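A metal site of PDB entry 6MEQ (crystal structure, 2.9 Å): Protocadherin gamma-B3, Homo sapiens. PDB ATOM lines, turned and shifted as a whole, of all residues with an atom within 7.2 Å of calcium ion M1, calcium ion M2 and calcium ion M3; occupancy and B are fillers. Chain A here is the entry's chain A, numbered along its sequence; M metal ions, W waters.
OE2 of Glu 114 lies close to N of Ala 205, at 2.9 Å.
OD1 of Asp 204 sits close to NE of Arg 172 (2.6 Å).
The side-chain carboxylate (OD2) of Asp 204 lies within hydrogen-bond range of the backbone NH (N) of Glu 241 (3.1 Å).
OE2 of Glu 173 lies close to NH1 of Arg 172.
The backbone carbonyl oxygen of Asn 206 is in hydrogen-bond range of a ring nitrogen (NE2) of His 297, at 3.4 Å.
O of Ala 203 lies within hydrogen-bond range of N of Glu 114, 3.3 Å away.
The side-chain carboxylate (OD2) of Asp 204 lies within hydrogen-bond range of the side-chain amide nitrogen (ND2) of Asn 244 (3.4 Å).
OD1 of Asp 293 sits at hydrogen-bond distance from N of His 297.
Three residues have an atom within 4 Å of calcium ion M1: Asp 171, Glu 173 and Asp 207.
The nearest printed residue that does not touch calcium ion M1 is Asn 208 (4.1 Å).
Of the 28 residues printed, 6 come within 4 Å of calcium ion M2.
The nearest printed residue that does not touch calcium ion M2 is Arg 172 (4.004 Å).
Of the 28 residues printed, 6 come within 4 Å of calcium ion M3.
Along chain A the residues within 4 Å of calcium ion M3 span positions 206 to 293.
Calcium ion M1 is bound by OE1 of Glu 173 (2.5 Å), OD2 of Asp 207 (2.5 Å), water W1 (2.5 Å) and OD1 of Asp 171 (2.5 Å).
Calcium ion M1 has four donor atoms within binding distance.
Calcium ion M2 is bound by OD1 of Asp 207 (2.4 Å), OD1 of Asp 204 (2.4 Å), OE2 of Glu 114 (2.4 Å), OE2 of Glu 173 (2.4 Å), OE1 of Glu 173 (2.6 Å) and OD1 of Asp 240 (2.8 Å).
Calcium ion M2 has six donor atoms within binding distance.
Slightly farther from calcium ion M2 lies O of Ala 205 (2.9 Å).
OD1 of Asn 206 binds calcium ion M3 (2.4 Å).
OD2 of Asp 238 binds calcium ion M3, 2.5 Å away.
Calcium ion M3 is bound by the backbone carbonyl oxygen (O) of Asn 208 (2.5 Å).
OD2 of Asp 240 binds calcium ion M3, at 2.5 Å.
OD1 of Asp 238 is bound to calcium ion M3 (2.6 Å).
O of Asn 244 binds calcium ion M3.
Calcium ion M3 is bound by the side-chain carboxylate (OD2) of Asp 293 (2.8 Å).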
ATOM      1  N   GLU A 114      16.726 -15.449 -19.342  1.00  0.00           N
ATOM      2  CA  GLU A 114      15.979 -16.678 -19.142  1.00  0.00           C
ATOM      3  C   GLU A 114      16.849 -17.830 -18.644  1.00  0.00           C
ATOM      4  O   GLU A 114      16.293 -18.855 -18.245  1.00  0.00           O
ATOM      5  CB  GLU A 114      15.283 -17.079 -20.450  1.00  0.00           C
ATOM      6  CG  GLU A 114      16.215 -17.273 -21.619  1.00  0.00           C
ATOM      7  CD  GLU A 114      15.485 -17.693 -22.877  1.00  0.00           C
ATOM      8  OE1 GLU A 114      14.270 -17.976 -22.806  1.00  0.00           O
ATOM      9  OE2 GLU A 114      16.127 -17.729 -23.952  1.00  0.00           O
ATOM     10  N   LEU A 170      12.188 -19.035 -16.217  1.00  0.00           N
ATOM     11  CA  LEU A 170      11.612 -18.134 -17.203  1.00  0.00           C
ATOM     12  C   LEU A 170      11.905 -18.621 -18.623  1.00  0.00           C
ATOM     13  O   LEU A 170      12.939 -19.236 -18.892  1.00  0.00           O
ATOM     14  CB  LEU A 170      12.166 -16.719 -17.027  1.00  0.00           C
ATOM     15  CG  LEU A 170      11.843 -16.020 -15.702  1.00  0.00           C
ATOM     16  CD1 LEU A 170      12.401 -14.610 -15.693  1.00  0.00           C
ATOM     17  CD2 LEU A 170      10.344 -16.011 -15.446  1.00  0.00           C
ATOM     18  N   ASP A 171      10.972 -18.332 -19.528  1.00  0.00           N
ATOM     19  CA  ASP A 171      11.080 -18.738 -20.929  1.00  0.00           C
ATOM     20  C   ASP A 171      10.517 -17.610 -21.788  1.00  0.00           C
ATOM     21  O   ASP A 171       9.316 -17.337 -21.742  1.00  0.00           O
ATOM     22  CB  ASP A 171      10.342 -20.048 -21.187  1.00  0.00           C
ATOM     23  CG  ASP A 171      10.605 -20.608 -22.576  1.00  0.00           C
ATOM     24  OD1 ASP A 171      11.440 -20.031 -23.308  1.00  0.00           O
ATOM     25  OD2 ASP A 171       9.974 -21.630 -22.935  1.00  0.00           O
ATOM     26  N   ARG A 172      11.397 -16.962 -22.567  1.00  0.00           N
ATOM     27  CA  ARG A 172      10.937 -15.873 -23.423  1.00  0.00           C
ATOM     28  C   ARG A 172      10.061 -16.395 -24.563  1.00  0.00           C
ATOM     29  O   ARG A 172       9.158 -15.689 -25.014  1.00  0.00           O
ATOM     30  CB  ARG A 172      12.134 -15.110 -23.980  1.00  0.00           C
ATOM     31  CG  ARG A 172      11.756 -13.853 -24.753  1.00  0.00           C
ATOM     32  CD  ARG A 172      12.917 -13.364 -25.598  1.00  0.00           C
ATOM     33  NE  ARG A 172      13.329 -14.366 -26.576  1.00  0.00           N
ATOM     34  CZ  ARG A 172      12.845 -14.449 -27.813  1.00  0.00           C
ATOM     35  NH1 ARG A 172      13.286 -15.393 -28.630  1.00  0.00           N
ATOM     36  NH2 ARG A 172      11.926 -13.583 -28.229  1.00  0.00           N
ATOM     37  N   GLU A 173      10.323 -17.616 -25.034  1.00  0.00           N
ATOM     38  CA  GLU A 173       9.516 -18.187 -26.108  1.00  0.00           C
ATOM     39  C   GLU A 173       8.095 -18.493 -25.667  1.00  0.00           C
ATOM     40  O   GLU A 173       7.229 -18.715 -26.521  1.00  0.00           O
ATOM     41  CB  GLU A 173      10.185 -19.449 -26.649  1.00  0.00           C
ATOM     42  CG  GLU A 173      11.339 -19.200 -27.620  1.00  0.00           C
ATOM     43  CD  GLU A 173      12.523 -18.495 -26.969  1.00  0.00           C
ATOM     44  OE1 GLU A 173      12.696 -18.616 -25.740  1.00  0.00           O
ATOM     45  OE2 GLU A 173      13.281 -17.828 -27.699  1.00  0.00           O
ATOM     46  N   GLU A 174       7.844 -18.526 -24.360  1.00  0.00           N
ATOM     47  CA  GLU A 174       6.494 -18.752 -23.820  1.00  0.00           C
ATOM     48  C   GLU A 174       5.837 -17.473 -23.320  1.00  0.00           C
ATOM     49  O   GLU A 174       4.661 -17.240 -23.595  1.00  0.00           O
ATOM     50  CB  GLU A 174       6.556 -19.778 -22.686  1.00  0.00           C
ATOM     51  CG  GLU A 174       5.191 -20.141 -22.111  1.00  0.00           C
ATOM     52  CD  GLU A 174       4.333 -20.935 -23.072  1.00  0.00           C
ATOM     53  OE1 GLU A 174       4.890 -21.528 -24.022  1.00  0.00           O
ATOM     54  OE2 GLU A 174       3.099 -20.969 -22.883  1.00  0.00           O
ATOM     55  N   ALA A 203      15.136 -11.412 -20.976  1.00  0.00           N
ATOM     56  CA  ALA A 203      16.176 -11.334 -21.991  1.00  0.00           C
ATOM     57  C   ALA A 203      16.362 -12.685 -22.674  1.00  0.00           C
ATOM     58  O   ALA A 203      16.201 -13.739 -22.057  1.00  0.00           O
ATOM     59  CB  ALA A 203      17.503 -10.872 -21.375  1.00  0.00           C
ATOM     60  N   ASP A 204      16.713 -12.637 -23.957  1.00  0.00           N
ATOM     61  CA  ASP A 204      16.794 -13.844 -24.771  1.00  0.00           C
ATOM     62  C   ASP A 204      18.177 -14.473 -24.664  1.00  0.00           C
ATOM     63  O   ASP A 204      19.196 -13.786 -24.718  1.00  0.00           O
ATOM     64  CB  ASP A 204      16.493 -13.529 -26.234  1.00  0.00           C
ATOM     65  CG  ASP A 204      16.451 -14.780 -27.093  1.00  0.00           C
ATOM     66  OD1 ASP A 204      15.587 -15.645 -26.845  1.00  0.00           O
ATOM     67  OD2 ASP A 204      17.281 -14.898 -28.024  1.00  0.00           O
ATOM     68  N   ALA A 205      18.193 -15.797 -24.501  1.00  0.00           N
ATOM     69  CA  ALA A 205      19.415 -16.581 -24.541  1.00  0.00           C
ATOM     70  C   ALA A 205      19.249 -17.692 -25.572  1.00  0.00           C
ATOM     71  O   ALA A 205      18.133 -18.112 -25.881  1.00  0.00           O
ATOM     72  CB  ALA A 205      19.766 -17.169 -23.169  1.00  0.00           C
ATOM     73  N   ASN A 206      20.379 -18.162 -26.093  1.00  0.00           N
ATOM     74  CA  ASN A 206      20.374 -19.187 -27.148  1.00  0.00           C
ATOM     75  C   ASN A 206      20.006 -20.528 -26.528  1.00  0.00           C
ATOM     76  O   ASN A 206      20.844 -21.398 -26.281  1.00  0.00           O
ATOM     77  CB  ASN A 206      21.728 -19.245 -27.851  1.00  0.00           C
ATOM     78  CG  ASN A 206      21.623 -19.785 -29.253  1.00  0.00           C
ATOM     79  OD1 ASN A 206      20.641 -19.555 -29.950  1.00  0.00           O
ATOM     80  ND2 ASN A 206      22.642 -20.522 -29.679  1.00  0.00           N
ATOM     81  N   ASP A 207      18.704 -20.695 -26.261  1.00  0.00           N
ATOM     82  CA  ASP A 207      18.178 -21.922 -25.658  1.00  0.00           C
ATOM     83  C   ASP A 207      17.443 -22.797 -26.664  1.00  0.00           C
ATOM     84  O   ASP A 207      16.628 -23.636 -26.276  1.00  0.00           O
ATOM     85  CB  ASP A 207      17.268 -21.569 -24.479  1.00  0.00           C
ATOM     86  CG  ASP A 207      16.045 -20.763 -24.899  1.00  0.00           C
ATOM     87  OD1 ASP A 207      16.105 -20.111 -25.963  1.00  0.00           O
ATOM     88  OD2 ASP A 207      15.036 -20.789 -24.169  1.00  0.00           O
ATOM     89  N   ASN A 208      17.708 -22.617 -27.961  1.00  0.00           N
ATOM     90  CA  ASN A 208      17.067 -23.421 -28.989  1.00  0.00           C
ATOM     91  C   ASN A 208      17.939 -23.477 -30.239  1.00  0.00           C
ATOM     92  O   ASN A 208      18.129 -22.453 -30.904  1.00  0.00           O
ATOM     93  CB  ASN A 208      15.686 -22.857 -29.324  1.00  0.00           C
ATOM     94  CG  ASN A 208      14.562 -23.796 -28.944  1.00  0.00           C
ATOM     95  OD1 ASN A 208      14.709 -25.017 -28.981  1.00  0.00           O
ATOM     96  ND2 ASN A 208      13.422 -23.234 -28.551  1.00  0.00           N
ATOM     97  N   PRO A 209      18.469 -24.637 -30.580  1.00  0.00           N
ATOM     98  CA  PRO A 209      19.303 -24.761 -31.777  1.00  0.00           C
ATOM     99  C   PRO A 209      18.450 -24.761 -33.031  1.00  0.00           C
ATOM    100  O   PRO A 209      17.229 -24.962 -32.954  1.00  0.00           O
ATOM    101  CB  PRO A 209      20.012 -26.105 -31.586  1.00  0.00           C
ATOM    102  CG  PRO A 209      19.057 -26.900 -30.762  1.00  0.00           C
ATOM    103  CD  PRO A 209      18.377 -25.914 -29.842  1.00  0.00           C
ATOM    104  N   PRO A 210      19.047 -24.523 -34.205  1.00  0.00           N
ATOM    105  CA  PRO A 210      18.267 -24.575 -35.447  1.00  0.00           C
ATOM    106  C   PRO A 210      17.714 -25.965 -35.705  1.00  0.00           C
ATOM    107  O   PRO A 210      18.322 -26.982 -35.331  1.00  0.00           O
ATOM    108  CB  PRO A 210      19.287 -24.169 -36.522  1.00  0.00           C
ATOM    109  CG  PRO A 210      20.335 -23.409 -35.779  1.00  0.00           C
ATOM    110  CD  PRO A 210      20.427 -24.054 -34.433  1.00  0.00           C
ATOM    111  N   ILE A 237      14.531 -23.497 -38.854  1.00  0.00           N
ATOM    112  CA  ILE A 237      13.720 -22.653 -37.992  1.00  0.00           C
ATOM    113  C   ILE A 237      14.434 -22.483 -36.663  1.00  0.00           C
ATOM    114  O   ILE A 237      14.894 -23.470 -36.068  1.00  0.00           O
ATOM    115  CB  ILE A 237      12.309 -23.239 -37.789  1.00  0.00           C
ATOM    116  CG1 ILE A 237      11.622 -23.446 -39.143  1.00  0.00           C
ATOM    117  CG2 ILE A 237      11.474 -22.333 -36.903  1.00  0.00           C
ATOM    118  CD1 ILE A 237      10.226 -24.026 -39.044  1.00  0.00           C
ATOM    119  N   ASP A 238      14.532 -21.233 -36.200  1.00  0.00           N
ATOM    120  CA  ASP A 238      15.151 -20.908 -34.921  1.00  0.00           C
ATOM    121  C   ASP A 238      14.177 -20.034 -34.135  1.00  0.00           C
ATOM    122  O   ASP A 238      13.758 -18.988 -34.615  1.00  0.00           O
ATOM    123  CB  ASP A 238      16.481 -20.195 -35.125  1.00  0.00           C
ATOM    124  CG  ASP A 238      17.397 -20.301 -33.912  1.00  0.00           C
ATOM    125  OD1 ASP A 238      16.880 -20.336 -32.773  1.00  0.00           O
ATOM    126  OD2 ASP A 238      18.629 -20.370 -34.101  1.00  0.00           O
ATOM    127  N   MET A 239      13.828 -20.477 -32.927  1.00  0.00           N
ATOM    128  CA  MET A 239      12.833 -19.805 -32.108  1.00  0.00           C
ATOM    129  C   MET A 239      13.405 -18.675 -31.265  1.00  0.00           C
ATOM    130  O   MET A 239      12.679 -18.093 -30.458  1.00  0.00           O
ATOM    131  CB  MET A 239      12.128 -20.822 -31.192  1.00  0.00           C
ATOM    132  CG  MET A 239      11.375 -21.908 -31.933  1.00  0.00           C
ATOM    133  SD  MET A 239      10.045 -21.248 -32.965  1.00  0.00           S
ATOM    134  CE  MET A 239       9.375 -22.760 -33.659  1.00  0.00           C
ATOM    135  N   ASP A 240      14.681 -18.349 -31.433  1.00  0.00           N
ATOM    136  CA  ASP A 240      15.325 -17.314 -30.633  1.00  0.00           C
ATOM    137  C   ASP A 240      15.193 -15.964 -31.337  1.00  0.00           C
ATOM    138  O   ASP A 240      14.486 -15.822 -32.335  1.00  0.00           O
ATOM    139  CB  ASP A 240      16.778 -17.695 -30.361  1.00  0.00           C
ATOM    140  CG  ASP A 240      16.902 -18.935 -29.501  1.00  0.00           C
ATOM    141  OD1 ASP A 240      16.060 -19.113 -28.607  1.00  0.00           O
ATOM    142  OD2 ASP A 240      17.844 -19.728 -29.720  1.00  0.00           O
ATOM    143  N   GLU A 241      15.868 -14.946 -30.795  1.00  0.00           N
ATOM    144  CA  GLU A 241      15.729 -13.579 -31.269  1.00  0.00           C
ATOM    145  C   GLU A 241      17.098 -12.936 -31.408  1.00  0.00           C
ATOM    146  O   GLU A 241      17.975 -13.123 -30.565  1.00  0.00           O
ATOM    147  CB  GLU A 241      14.874 -12.745 -30.299  1.00  0.00           C
ATOM    148  CG  GLU A 241      14.696 -11.288 -30.700  1.00  0.00           C
ATOM    149  CD  GLU A 241      13.961 -10.479 -29.640  1.00  0.00           C
ATOM    150  OE1 GLU A 241      13.624 -11.053 -28.580  1.00  0.00           O
ATOM    151  OE2 GLU A 241      13.725  -9.274 -29.868  1.00  0.00           O
ATOM    152  N   ILE A 243      20.797 -12.126 -32.751  1.00  0.00           N
ATOM    153  CA  ILE A 243      21.921 -12.887 -33.285  1.00  0.00           C
ATOM    154  C   ILE A 243      21.718 -14.377 -33.081  1.00  0.00           C
ATOM    155  O   ILE A 243      22.204 -15.205 -33.872  1.00  0.00           O
ATOM    156  CB  ILE A 243      23.244 -12.386 -32.654  1.00  0.00           C
ATOM    157  CG1 ILE A 243      24.441 -13.149 -33.223  1.00  0.00           C
ATOM    158  CG2 ILE A 243      23.195 -12.528 -31.137  1.00  0.00           C
ATOM    159  CD1 ILE A 243      24.626 -12.983 -34.716  1.00  0.00           C
ATOM    160  N   ASN A 244      20.993 -14.768 -32.027  1.00  0.00           N
ATOM    161  CA  ASN A 244      20.708 -16.163 -31.753  1.00  0.00           C
ATOM    162  C   ASN A 244      19.699 -16.762 -32.723  1.00  0.00           C
ATOM    163  O   ASN A 244      19.373 -17.955 -32.590  1.00  0.00           O
ATOM    164  CB  ASN A 244      20.207 -16.329 -30.321  1.00  0.00           C
ATOM    165  CG  ASN A 244      21.192 -15.799 -29.297  1.00  0.00           C
ATOM    166  OD1 ASN A 244      22.410 -15.815 -29.519  1.00  0.00           O
ATOM    167  ND2 ASN A 244      20.675 -15.329 -28.169  1.00  0.00           N
ATOM    168  N   ALA A 245      19.194 -15.990 -33.680  1.00  0.00           N
ATOM    169  CA  ALA A 245      18.232 -16.475 -34.659  1.00  0.00           C
ATOM    170  C   ALA A 245      18.746 -16.467 -36.092  1.00  0.00           C
ATOM    171  O   ALA A 245      18.181 -17.167 -36.941  1.00  0.00           O
ATOM    172  CB  ALA A 245      16.926 -15.666 -34.603  1.00  0.00           C
ATOM    173  N   GLU A 246      19.797 -15.693 -36.387  1.00  0.00           N
ATOM    174  CA  GLU A 246      20.349 -15.677 -37.737  1.00  0.00           C
ATOM    175  C   GLU A 246      21.031 -16.998 -38.042  1.00  0.00           C
ATOM    176  O   GLU A 246      21.893 -17.463 -37.276  1.00  0.00           O
ATOM    177  CB  GLU A 246      21.335 -14.515 -37.878  1.00  0.00           C
ATOM    178  CG  GLU A 246      20.730 -13.145 -37.594  1.00  0.00           C
ATOM    179  CD  GLU A 246      21.750 -12.032 -37.678  1.00  0.00           C
ATOM    180  OE1 GLU A 246      22.919 -12.319 -37.992  1.00  0.00           O
ATOM    181  OE2 GLU A 246      21.378 -10.865 -37.443  1.00  0.00           O
ATOM    182  N   ILE A 247      20.657 -17.620 -39.161  1.00  0.00           N
ATOM    183  CA  ILE A 247      21.129 -18.947 -39.531  1.00  0.00           C
ATOM    184  C   ILE A 247      21.941 -18.839 -40.811  1.00  0.00           C
ATOM    185  O   ILE A 247      21.527 -18.150 -41.758  1.00  0.00           O
ATOM    186  CB  ILE A 247      19.962 -19.930 -39.701  1.00  0.00           C
ATOM    187  CG1 ILE A 247      19.119 -19.991 -38.431  1.00  0.00           C
ATOM    188  CG2 ILE A 247      20.484 -21.320 -40.059  1.00  0.00           C
ATOM    189  CD1 ILE A 247      17.924 -20.909 -38.526  1.00  0.00           C
ATOM    190  N   ASP A 293      24.199 -20.842 -35.987  1.00  0.00           N
ATOM    191  CA  ASP A 293      23.583 -19.602 -35.529  1.00  0.00           C
ATOM    192  C   ASP A 293      24.593 -18.735 -34.788  1.00  0.00           C
ATOM    193  O   ASP A 293      25.801 -18.935 -34.936  1.00  0.00           O
ATOM    194  CB  ASP A 293      22.373 -19.898 -34.628  1.00  0.00           C
ATOM    195  CG  ASP A 293      22.731 -20.754 -33.415  1.00  0.00           C
ATOM    196  OD1 ASP A 293      23.899 -21.192 -33.321  1.00  0.00           O
ATOM    197  OD2 ASP A 293      21.852 -20.975 -32.567  1.00  0.00           O
ATOM    198  N   GLY A 294      24.107 -17.768 -34.016  1.00  0.00           N
ATOM    199  CA  GLY A 294      25.003 -16.890 -33.284  1.00  0.00           C
ATOM    200  C   GLY A 294      25.689 -17.563 -32.118  1.00  0.00           C
ATOM    201  O   GLY A 294      26.850 -17.272 -31.816  1.00  0.00           O
ATOM    202  N   GLY A 295      24.996 -18.478 -31.445  1.00  0.00           N
ATOM    203  CA  GLY A 295      25.560 -19.177 -30.303  1.00  0.00           C
ATOM    204  C   GLY A 295      26.288 -20.445 -30.677  1.00  0.00           C
ATOM    205  O   GLY A 295      26.521 -21.310 -29.825  1.00  0.00           O
ATOM    206  N   HIS A 297      25.316 -23.002 -32.282  1.00  0.00           N
ATOM    207  CA  HIS A 297      24.525 -24.219 -32.253  1.00  0.00           C
ATOM    208  C   HIS A 297      24.411 -24.786 -33.659  1.00  0.00           C
ATOM    209  O   HIS A 297      24.041 -24.077 -34.604  1.00  0.00           O
ATOM    210  CB  HIS A 297      23.135 -23.954 -31.668  1.00  0.00           C
ATOM    211  CG  HIS A 297      23.108 -23.885 -30.173  1.00  0.00           C
ATOM    212  ND1 HIS A 297      24.245 -24.015 -29.402  1.00  0.00           N
ATOM    213  CD2 HIS A 297      22.082 -23.713 -29.310  1.00  0.00           C
ATOM    214  CE1 HIS A 297      23.923 -23.919 -28.125  1.00  0.00           C
ATOM    215  NE2 HIS A 297      22.618 -23.729 -28.040  1.00  0.00           N
HETATM  216 CA    CA M   1      12.771 -21.016 -25.189  1.00  0.00          CA
HETATM  217 CA    CA M   2      15.211 -17.929 -26.202  1.00  0.00          CA
HETATM  218 CA    CA M   3      19.223 -20.382 -31.710  1.00  0.00          CA
HETATM  219  O   HOH W   1      12.355 -23.196 -24.032  1.00  0.00           O
HETATM  220  O   HOH W   2      13.878 -21.903 -22.100  1.00  0.00           O
